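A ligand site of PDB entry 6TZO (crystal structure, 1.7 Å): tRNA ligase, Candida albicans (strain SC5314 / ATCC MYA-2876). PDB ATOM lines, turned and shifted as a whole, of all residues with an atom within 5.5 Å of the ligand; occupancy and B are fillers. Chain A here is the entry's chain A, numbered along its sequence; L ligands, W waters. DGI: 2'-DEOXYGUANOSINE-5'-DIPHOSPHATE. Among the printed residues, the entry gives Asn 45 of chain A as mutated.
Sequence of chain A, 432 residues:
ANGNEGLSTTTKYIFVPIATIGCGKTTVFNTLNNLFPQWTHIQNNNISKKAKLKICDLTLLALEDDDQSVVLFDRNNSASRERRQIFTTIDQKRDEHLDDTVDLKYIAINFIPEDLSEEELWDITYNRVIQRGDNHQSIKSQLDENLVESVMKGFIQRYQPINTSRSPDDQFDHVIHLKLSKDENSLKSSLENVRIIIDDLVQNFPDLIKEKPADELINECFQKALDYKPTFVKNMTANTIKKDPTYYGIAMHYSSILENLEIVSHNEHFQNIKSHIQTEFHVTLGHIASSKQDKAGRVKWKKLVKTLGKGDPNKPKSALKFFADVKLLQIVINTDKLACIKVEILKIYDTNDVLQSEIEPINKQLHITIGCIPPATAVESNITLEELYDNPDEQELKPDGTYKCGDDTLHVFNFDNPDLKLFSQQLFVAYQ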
ATOM      1  N   THR A  20     -31.749  23.091  29.025  1.00  0.00           N
ATOM      2  CA  THR A  20     -30.942  21.913  28.742  1.00  0.00           C
ATOM      3  C   THR A  20     -29.485  22.346  28.615  1.00  0.00           C
ATOM      4  O   THR A  20     -29.164  23.522  28.761  1.00  0.00           O
ATOM      5  CB  THR A  20     -31.423  21.188  27.476  1.00  0.00           C
ATOM      6  OG1 THR A  20     -31.384  22.102  26.376  1.00  0.00           O
ATOM      7  CG2 THR A  20     -32.847  20.662  27.656  1.00  0.00           C
ATOM      8  N   ILE A  21     -28.588  21.391  28.400  1.00  0.00           N
ATOM      9  CA  ILE A  21     -27.173  21.737  28.389  1.00  0.00           C
ATOM     10  C   ILE A  21     -26.870  22.693  27.250  1.00  0.00           C
ATOM     11  O   ILE A  21     -27.356  22.518  26.121  1.00  0.00           O
ATOM     12  CB  ILE A  21     -26.319  20.457  28.275  1.00  0.00           C
ATOM     13  CG1 ILE A  21     -26.530  19.605  29.525  1.00  0.00           C
ATOM     14  CG2 ILE A  21     -24.863  20.814  28.052  1.00  0.00           C
ATOM     15  CD1 ILE A  21     -25.826  18.261  29.437  1.00  0.00           C
ATOM     16  N   GLY A  22     -26.066  23.708  27.528  1.00  0.00           N
ATOM     17  CA  GLY A  22     -25.603  24.623  26.498  1.00  0.00           C
ATOM     18  C   GLY A  22     -26.549  25.771  26.175  1.00  0.00           C
ATOM     19  O   GLY A  22     -26.284  26.504  25.222  1.00  0.00           O
ATOM     20  N   CYS A  23     -27.640  25.928  26.936  1.00  0.00           N
ATOM     21  CA  CYS A  23     -28.553  27.038  26.688  1.00  0.00           C
ATOM     22  C   CYS A  23     -27.977  28.383  27.127  1.00  0.00           C
ATOM     23  O   CYS A  23     -28.540  29.426  26.779  1.00  0.00           O
ATOM     24  CB  CYS A  23     -29.902  26.812  27.387  1.00  0.00           C
ATOM     25  SG  CYS A  23     -30.941  25.569  26.628  1.00  0.00           S
ATOM     26  N   GLY A  24     -26.910  28.373  27.919  1.00  0.00           N
ATOM     27  CA  GLY A  24     -26.269  29.577  28.371  1.00  0.00           C
ATOM     28  C   GLY A  24     -26.529  29.942  29.818  1.00  0.00           C
ATOM     29  O   GLY A  24     -26.319  31.102  30.175  1.00  0.00           O
ATOM     30  N   LYS A  25     -26.967  28.993  30.645  1.00  0.00           N
ATOM     31  CA  LYS A  25     -27.215  29.252  32.058  1.00  0.00           C
ATOM     32  C   LYS A  25     -25.986  29.830  32.741  1.00  0.00           C
ATOM     33  O   LYS A  25     -26.060  30.880  33.400  1.00  0.00           O
ATOM     34  CB  LYS A  25     -27.615  27.968  32.787  1.00  0.00           C
ATOM     35  CG  LYS A  25     -28.864  27.296  32.299  1.00  0.00           C
ATOM     36  CD  LYS A  25     -29.153  26.057  33.166  1.00  0.00           C
ATOM     37  CE  LYS A  25     -28.057  24.969  33.033  1.00  0.00           C
ATOM     38  NZ  LYS A  25     -27.899  24.392  31.640  1.00  0.00           N
ATOM     39  N   THR A  26     -24.852  29.137  32.625  1.00  0.00           N
ATOM     40  CA  THR A  26     -23.660  29.565  33.353  1.00  0.00           C
ATOM     41  C   THR A  26     -23.204  30.947  32.879  1.00  0.00           C
ATOM     42  O   THR A  26     -22.822  31.789  33.696  1.00  0.00           O
ATOM     43  CB  THR A  26     -22.552  28.525  33.178  1.00  0.00           C
ATOM     44  OG1 THR A  26     -22.987  27.273  33.707  1.00  0.00           O
ATOM     45  CG2 THR A  26     -21.269  28.964  33.902  1.00  0.00           C
ATOM     46  N   THR A  27     -23.298  31.207  31.571  1.00  0.00           N
ATOM     47  CA  THR A  27     -22.873  32.489  31.024  1.00  0.00           C
ATOM     48  C   THR A  27     -23.774  33.625  31.492  1.00  0.00           C
ATOM     49  O   THR A  27     -23.284  34.677  31.914  1.00  0.00           O
ATOM     50  CB  THR A  27     -22.852  32.433  29.497  1.00  0.00           C
ATOM     51  OG1 THR A  27     -21.988  31.369  29.070  1.00  0.00           O
ATOM     52  CG2 THR A  27     -22.335  33.771  28.896  1.00  0.00           C
ATOM     53  N   VAL A  28     -25.092  33.411  31.419  1.00  0.00           N
ATOM     54  CA  VAL A  28     -26.039  34.420  31.865  1.00  0.00           C
ATOM     55  C   VAL A  28     -25.882  34.689  33.357  1.00  0.00           C
ATOM     56  O   VAL A  28     -25.833  35.842  33.811  1.00  0.00           O
ATOM     57  CB  VAL A  28     -27.481  33.978  31.520  1.00  0.00           C
ATOM     58  CG1 VAL A  28     -28.500  34.854  32.232  1.00  0.00           C
ATOM     59  CG2 VAL A  28     -27.701  34.017  29.990  1.00  0.00           C
ATOM     60  N   ASN A  45     -22.815  22.186  38.730  1.00  0.00           N
ATOM     61  CA  ASN A  45     -21.609  21.624  38.133  1.00  0.00           C
ATOM     62  C   ASN A  45     -20.498  21.472  39.159  1.00  0.00           C
ATOM     63  O   ASN A  45     -19.656  20.565  39.025  1.00  0.00           O
ATOM     64  CB  ASN A  45     -21.079  22.523  37.007  1.00  0.00           C
ATOM     65  CG  ASN A  45     -22.077  22.752  35.894  1.00  0.00           C
ATOM     66  OD1 ASN A  45     -22.958  21.934  35.652  1.00  0.00           O
ATOM     67  ND2 ASN A  45     -21.935  23.883  35.193  1.00  0.00           N
ATOM     68  N   ASP A  74     -28.128  27.309  39.653  1.00  0.00           N
ATOM     69  CA  ASP A  74     -27.623  26.958  38.320  1.00  0.00           C
ATOM     70  C   ASP A  74     -27.674  25.437  38.128  1.00  0.00           C
ATOM     71  O   ASP A  74     -26.728  24.714  38.425  1.00  0.00           O
ATOM     72  CB  ASP A  74     -26.213  27.485  38.122  1.00  0.00           C
ATOM     73  CG  ASP A  74     -25.781  27.497  36.651  1.00  0.00           C
ATOM     74  OD1 ASP A  74     -26.319  26.719  35.845  1.00  0.00           O
ATOM     75  OD2 ASP A  74     -24.874  28.282  36.320  1.00  0.00           O
ATOM     76  N   ASN A  76     -30.111  22.550  35.304  1.00  0.00           N
ATOM     77  CA  ASN A  76     -30.967  22.557  34.113  1.00  0.00           C
ATOM     78  C   ASN A  76     -32.446  22.551  34.469  1.00  0.00           C
ATOM     79  O   ASN A  76     -33.231  23.301  33.891  1.00  0.00           O
ATOM     80  CB  ASN A  76     -30.667  21.347  33.236  1.00  0.00           C
ATOM     81  CG  ASN A  76     -29.476  21.555  32.370  1.00  0.00           C
ATOM     82  OD1 ASN A  76     -29.485  22.437  31.511  1.00  0.00           O
ATOM     83  ND2 ASN A  76     -28.449  20.765  32.579  1.00  0.00           N
ATOM     84  N   ARG A 128     -22.864  24.887  20.127  1.00  0.00           N
ATOM     85  CA  ARG A 128     -22.221  25.660  21.187  1.00  0.00           C
ATOM     86  C   ARG A 128     -21.275  24.792  22.002  1.00  0.00           C
ATOM     87  O   ARG A 128     -20.150  25.211  22.321  1.00  0.00           O
ATOM     88  CB  ARG A 128     -23.273  26.256  22.116  1.00  0.00           C
ATOM     89  CG  ARG A 128     -23.821  27.564  21.686  1.00  0.00           C
ATOM     90  CD  ARG A 128     -24.790  28.038  22.730  1.00  0.00           C
ATOM     91  NE  ARG A 128     -25.521  29.204  22.284  1.00  0.00           N
ATOM     92  CZ  ARG A 128     -26.510  29.745  22.979  1.00  0.00           C
ATOM     93  NH1 ARG A 128     -26.868  29.211  24.143  1.00  0.00           N
ATOM     94  NH2 ARG A 128     -27.139  30.802  22.513  1.00  0.00           N
ATOM     95  N   VAL A 129     -21.711  23.597  22.373  1.00  0.00           N
ATOM     96  CA  VAL A 129     -20.942  22.798  23.319  1.00  0.00           C
ATOM     97  C   VAL A 129     -19.704  22.205  22.655  1.00  0.00           C
ATOM     98  O   VAL A 129     -18.630  22.186  23.250  1.00  0.00           O
ATOM     99  CB  VAL A 129     -21.835  21.711  23.956  1.00  0.00           C
ATOM    100  CG1 VAL A 129     -20.999  20.661  24.658  1.00  0.00           C
ATOM    101  CG2 VAL A 129     -22.817  22.352  24.934  1.00  0.00           C
ATOM    102  N   ARG A 132     -17.318  25.406  21.701  1.00  0.00           N
ATOM    103  CA  ARG A 132     -16.868  26.276  22.764  1.00  0.00           C
ATOM    104  C   ARG A 132     -16.718  25.583  24.109  1.00  0.00           C
ATOM    105  O   ARG A 132     -16.183  26.203  25.035  1.00  0.00           O
ATOM    106  CB  ARG A 132     -17.833  27.459  22.934  1.00  0.00           C
ATOM    107  CG  ARG A 132     -17.638  28.539  21.891  1.00  0.00           C
ATOM    108  CD  ARG A 132     -17.774  29.926  22.488  1.00  0.00           C
ATOM    109  NE  ARG A 132     -18.099  30.891  21.477  1.00  0.00           N
ATOM    110  CZ  ARG A 132     -17.383  31.992  21.323  1.00  0.00           C
ATOM    111  NH1 ARG A 132     -16.332  32.263  22.128  1.00  0.00           N
ATOM    112  NH2 ARG A 132     -17.700  32.885  20.416  1.00  0.00           N
ATOM    113  N   GLY A 133     -17.192  24.369  24.250  1.00  0.00           N
ATOM    114  CA  GLY A 133     -17.064  23.645  25.489  1.00  0.00           C
ATOM    115  C   GLY A 133     -18.179  23.958  26.476  1.00  0.00           C
ATOM    116  O   GLY A 133     -18.896  24.943  26.360  1.00  0.00           O
ATOM    117  N   ASP A 134     -18.323  23.076  27.454  1.00  0.00           N
ATOM    118  CA  ASP A 134     -19.317  23.243  28.500  1.00  0.00           C
ATOM    119  C   ASP A 134     -18.733  22.697  29.800  1.00  0.00           C
ATOM    120  O   ASP A 134     -17.808  21.892  29.790  1.00  0.00           O
ATOM    121  CB  ASP A 134     -20.623  22.524  28.137  1.00  0.00           C
ATOM    122  CG  ASP A 134     -21.809  23.070  28.890  1.00  0.00           C
ATOM    123  OD1 ASP A 134     -22.124  22.520  29.976  1.00  0.00           O
ATOM    124  OD2 ASP A 134     -22.425  24.039  28.407  1.00  0.00           O
ATOM    125  N   ASN A 135     -19.286  23.166  30.914  1.00  0.00           N
ATOM    126  CA  ASN A 135     -18.763  22.807  32.217  1.00  0.00           C
ATOM    127  C   ASN A 135     -19.640  21.791  32.955  1.00  0.00           C
ATOM    128  O   ASN A 135     -19.340  21.456  34.107  1.00  0.00           O
ATOM    129  CB  ASN A 135     -18.571  24.069  33.070  1.00  0.00           C
ATOM    130  CG  ASN A 135     -17.223  24.728  32.810  1.00  0.00           C
ATOM    131  OD1 ASN A 135     -16.771  25.571  33.592  1.00  0.00           O
ATOM    132  ND2 ASN A 135     -16.569  24.343  31.717  1.00  0.00           N
ATOM    133  N   ASP A 183     -26.662  33.609  16.990  1.00  0.00           N
ATOM    134  CA  ASP A 183     -26.286  34.990  17.196  1.00  0.00           C
ATOM    135  C   ASP A 183     -26.548  35.740  15.899  1.00  0.00           C
ATOM    136  O   ASP A 183     -26.289  35.236  14.804  1.00  0.00           O
ATOM    137  CB  ASP A 183     -24.824  35.088  17.635  1.00  0.00           C
ATOM    138  CG  ASP A 183     -24.493  34.146  18.812  1.00  0.00           C
ATOM    139  OD1 ASP A 183     -25.256  34.124  19.806  1.00  0.00           O
ATOM    140  OD2 ASP A 183     -23.473  33.443  18.742  1.00  0.00           O
ATOM    141  N   LYS A 188     -24.694  38.424  20.926  1.00  0.00           N
ATOM    142  CA  LYS A 188     -24.857  37.087  21.475  1.00  0.00           C
ATOM    143  C   LYS A 188     -26.228  36.940  22.134  1.00  0.00           C
ATOM    144  O   LYS A 188     -26.713  37.843  22.820  1.00  0.00           O
ATOM    145  CB  LYS A 188     -23.749  36.801  22.495  1.00  0.00           C
ATOM    146  CG  LYS A 188     -22.565  36.018  21.944  1.00  0.00           C
ATOM    147  CD  LYS A 188     -21.975  36.653  20.717  1.00  0.00           C
ATOM    148  CE  LYS A 188     -20.784  35.864  20.206  1.00  0.00           C
ATOM    149  NZ  LYS A 188     -19.615  36.048  21.106  1.00  0.00           N
ATOM    150  N   SER A 189     -26.853  35.799  21.881  1.00  0.00           N
ATOM    151  CA  SER A 189     -28.157  35.481  22.450  1.00  0.00           C
ATOM    152  C   SER A 189     -28.153  35.656  23.969  1.00  0.00           C
ATOM    153  O   SER A 189     -29.049  36.281  24.541  1.00  0.00           O
ATOM    154  CB  SER A 189     -28.519  34.048  22.039  1.00  0.00           C
ATOM    155  OG  SER A 189     -29.757  33.618  22.553  1.00  0.00           O
ATOM    156  N   SER A 190     -27.098  35.155  24.619  1.00  0.00           N
ATOM    157  CA  SER A 190     -27.028  35.217  26.083  1.00  0.00           C
ATOM    158  C   SER A 190     -26.956  36.650  26.594  1.00  0.00           C
ATOM    159  O   SER A 190     -27.496  36.942  27.657  1.00  0.00           O
ATOM    160  CB  SER A 190     -25.830  34.419  26.602  1.00  0.00           C
ATOM    161  OG  SER A 190     -26.075  33.021  26.503  1.00  0.00           O
ATOM    162  N   LEU A 191     -26.277  37.546  25.854  1.00  0.00           N
ATOM    163  CA  LEU A 191     -26.253  38.952  26.246  1.00  0.00           C
ATOM    164  C   LEU A 191     -27.633  39.570  26.102  1.00  0.00           C
ATOM    165  O   LEU A 191     -28.072  40.322  26.972  1.00  0.00           O
ATOM    166  CB  LEU A 191     -25.233  39.725  25.400  1.00  0.00           C
ATOM    167  CG  LEU A 191     -25.183  41.251  25.627  1.00  0.00           C
ATOM    168  CD1 LEU A 191     -24.924  41.615  27.099  1.00  0.00           C
ATOM    169  CD2 LEU A 191     -24.152  41.934  24.719  1.00  0.00           C
ATOM    170  N   PHE A 222     -20.474  40.905  30.562  1.00  0.00           N
ATOM    171  CA  PHE A 222     -20.758  39.754  29.716  1.00  0.00           C
ATOM    172  C   PHE A 222     -19.499  39.281  28.990  1.00  0.00           C
ATOM    173  O   PHE A 222     -19.246  38.066  28.903  1.00  0.00           O
ATOM    174  CB  PHE A 222     -21.840  40.125  28.698  1.00  0.00           C
ATOM    175  CG  PHE A 222     -22.131  39.026  27.739  1.00  0.00           C
ATOM    176  CD1 PHE A 222     -22.908  37.944  28.124  1.00  0.00           C
ATOM    177  CD2 PHE A 222     -21.605  39.059  26.447  1.00  0.00           C
ATOM    178  CE1 PHE A 222     -23.170  36.913  27.239  1.00  0.00           C
ATOM    179  CE2 PHE A 222     -21.880  38.030  25.566  1.00  0.00           C
ATOM    180  CZ  PHE A 222     -22.654  36.961  25.955  1.00  0.00           C
ATOM    181  N   LEU A 226     -17.920  35.594  29.145  1.00  0.00           N
ATOM    182  CA  LEU A 226     -17.806  34.868  27.900  1.00  0.00           C
ATOM    183  C   LEU A 226     -16.395  34.365  27.696  1.00  0.00           C
ATOM    184  O   LEU A 226     -16.196  33.243  27.225  1.00  0.00           O
ATOM    185  CB  LEU A 226     -18.243  35.771  26.756  1.00  0.00           C
ATOM    186  CG  LEU A 226     -18.792  35.157  25.478  1.00  0.00           C
ATOM    187  CD1 LEU A 226     -19.924  34.217  25.769  1.00  0.00           C
ATOM    188  CD2 LEU A 226     -19.224  36.280  24.576  1.00  0.00           C
ATOM    189  N   LYS A 229     -12.443  30.690  30.480  1.00  0.00           N
ATOM    190  CA  LYS A 229     -12.158  29.359  29.955  1.00  0.00           C
ATOM    191  C   LYS A 229     -11.459  28.531  31.027  1.00  0.00           C
ATOM    192  O   LYS A 229     -10.220  28.550  31.129  1.00  0.00           O
ATOM    193  CB  LYS A 229     -11.292  29.455  28.695  1.00  0.00           C
ATOM    194  CG  LYS A 229     -12.057  29.722  27.404  1.00  0.00           C
ATOM    195  CD  LYS A 229     -13.376  28.961  27.334  1.00  0.00           C
ATOM    196  CE  LYS A 229     -13.968  29.012  25.923  1.00  0.00           C
ATOM    197  NZ  LYS A 229     -15.453  29.001  25.930  1.00  0.00           N
HETATM  198  O1B DGI L   1     -24.451  26.461  31.481  1.00  0.00           O
HETATM  199  PB  DGI L   1     -24.952  26.015  30.139  1.00  0.00           P
HETATM  200  O2B DGI L   1     -24.565  24.567  29.894  1.00  0.00           O
HETATM  201  O3B DGI L   1     -26.462  26.148  30.019  1.00  0.00           O
HETATM  202  O3A DGI L   1     -24.395  26.956  28.952  1.00  0.00           O
HETATM  203  PA  DGI L   1     -23.043  27.790  28.984  1.00  0.00           P
HETATM  204  O1A DGI L   1     -23.273  29.170  29.577  1.00  0.00           O
HETATM  205  O2A DGI L   1     -21.895  27.020  29.622  1.00  0.00           O
HETATM  206  O5' DGI L   1     -22.746  27.981  27.426  1.00  0.00           O
HETATM  207  C5' DGI L   1     -22.314  26.854  26.671  1.00  0.00           C
HETATM  208  C4' DGI L   1     -21.232  27.343  25.715  1.00  0.00           C
HETATM  209  O4' DGI L   1     -21.794  28.269  24.792  1.00  0.00           O
HETATM  210  C3' DGI L   1     -20.110  28.074  26.427  1.00  0.00           C
HETATM  211  O3' DGI L   1     -18.880  27.667  25.804  1.00  0.00           O
HETATM  212  C2' DGI L   1     -20.315  29.551  26.148  1.00  0.00           C
HETATM  213  C1' DGI L   1     -21.134  29.535  24.879  1.00  0.00           C
HETATM  214  N9  DGI L   1     -22.228  30.523  24.871  1.00  0.00           N
HETATM  215  C8  DGI L   1     -23.044  30.919  25.878  1.00  0.00           C
HETATM  216  N7  DGI L   1     -23.953  31.835  25.441  1.00  0.00           N
HETATM  217  C5  DGI L   1     -23.710  32.001  24.106  1.00  0.00           C
HETATM  218  C4  DGI L   1     -22.593  31.124  23.766  1.00  0.00           C
HETATM  219  N3  DGI L   1     -22.113  31.069  22.499  1.00  0.00           N
HETATM  220  C2  DGI L   1     -22.684  31.834  21.562  1.00  0.00           C
HETATM  221  N2  DGI L   1     -22.166  31.744  20.303  1.00  0.00           N
HETATM  222  N1  DGI L   1     -23.727  32.650  21.796  1.00  0.00           N
HETATM  223  C6  DGI L   1     -24.286  32.793  23.011  1.00  0.00           C
HETATM  224  O6  DGI L   1     -25.256  33.558  23.212  1.00  0.00           O
HETATM  225  O   HOH W   1     -25.843  22.624  31.726  1.00  0.00           O
HETATM  226  O   HOH W   2     -19.339  28.101  30.273  1.00  0.00           O
HETATM  227  O   HOH W   3     -21.278  25.615  31.837  1.00  0.00           O
HETATM  228  O   HOH W   4     -24.853  29.946  19.350  1.00  0.00           O
HETATM  229  O   HOH W   5     -24.869  25.214  34.168  1.00  0.00           O
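NZ of Lys 25 lies within salt-bridge range of O3B of the ligand, at 2.8 Å. O3B of the ligand is in hydrogen-bond range of N of Lys 25, 3.0 Å away. An oxygen (O3A) of the ligand sits at hydrogen-bond distance from the backbone NH (N) of Gly 24 (3.1 Å). An oxygen (O1B) of the ligand lies within hydrogen-bond range of the side-chain hydroxyl (OG1) of Thr 26, 2.8 Å away. A nitrogen (N2) of the ligand sits at hydrogen-bond distance from the side-chain carboxylate of Asp 183 (2.7 Å). An oxygen (O6) of the ligand sits at hydrogen-bond distance from the guanidinium group (NH2) of Arg 128, at 3.4 Å. The backbone NH of Cys 23 sits at hydrogen-bond distance from an oxygen (O3B) of the ligand (3.3 Å). The side-chain hydroxyl (OG) of Ser 190 is in hydrogen-bond range of a nitrogen (N7) of the ligand. An oxygen (O2B) of the ligand is in hydrogen-bond range of the backbone NH (N) of Gly 22 (2.9 Å). An oxygen (O6) of the ligand is in hydrogen-bond range of the backbone NH of Ser 189 (3.1 Å). N of Thr 26 lies within hydrogen-bond range of O1B of the ligand (2.9 Å). An oxygen (O3') of the ligand sits close to the backbone carbonyl oxygen of Arg 132 (3.2 Å). The backbone NH of Thr 27 sits at hydrogen-bond distance from an oxygen (O1A) of the ligand. An oxygen (O6) of the ligand sits at hydrogen-bond distance from the backbone NH of Ser 190, at 2.8 Å. The side-chain hydroxyl (OG1) of Thr 27 lies within hydrogen-bond range of an oxygen (O1A) of the ligand (2.6 Å). An oxygen (O3') of the ligand sits at hydrogen-bond distance from the backbone carbonyl oxygen (O) of Gly 133 (2.8 Å). OD2 of Asp 134 lies close to O2B of the ligand, 2.7 Å away.
O of Thr 20 touches O3B of the ligand, at 3.97 Å. Ile 21 touches the ligand (C to O2B, 3.98 Å). Lys 188 touches the ligand (CG to N1, 3.6 Å). NZ of Lys 229 touches O3' of the ligand, 3.7 Å away. Within 4 Å of the ligand: Thr 20, Ile 21, Gly 22, Cys 23, Gly 24, Lys 25, Thr 26, Thr 27, Arg 128, Arg 132, Gly 133, Asp 134, Asp 183, Lys 188, Ser 189, Ser 190 and Lys 229.
The backbone carbonyl oxygen of Thr 20 is in hydrogen-bond range of the side-chain sulfur of Cys 23, at 3.4 Å. The side-chain amide oxygen (OD1) of Asn 76 sits close to the backbone carbonyl oxygen (O) of Thr 20. OG1 of Thr 26 lies within hydrogen-bond range of OD2 of Asp 74. NZ of Lys 229 is in hydrogen-bond range of O of Arg 132 (3.0 Å). The backbone carbonyl oxygen (O) of Gly 22 lies within hydrogen-bond range of the guanidinium group (NH1) of Arg 128, 3.0 Å away. The side-chain amino group of Lys 25 sits at hydrogen-bond distance from the side-chain amide oxygen of Asn 76 (2.5 Å). The backbone carbonyl oxygen (O) of Thr 20 is in hydrogen-bond range of the side-chain amino group (NZ) of Lys 25 (3.3 Å). The side-chain amide oxygen of Asn 76 sits at hydrogen-bond distance from the backbone NH of Ile 21, 3.4 Å away.
Water W3 lies within hydrogen-bond range of an oxygen (O2A) of the ligand (2.7 Å), the side-chain hydroxyl of Thr 26 (3.0 Å) and the backbone NH of Asn 135 (3.3 Å). Water W1 lies within hydrogen-bond range of the side-chain amino group of Lys 25 (2.7 Å), an oxygen (O2B) of the ligand (3.0 Å) and the side-chain amide nitrogen of Asn 76 (3.3 Å). Water W5 lies within hydrogen-bond range of OD1 of Asp 74 (2.7 Å), OG1 of Thr 26 (2.8 Å), O1B of the ligand (3.0 Å) and ND2 of Asn 45 (3.4 Å). Water W4 lies within hydrogen-bond range of NE of Arg 128 (3.1 Å) and N2 of the ligand (3.4 Å).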
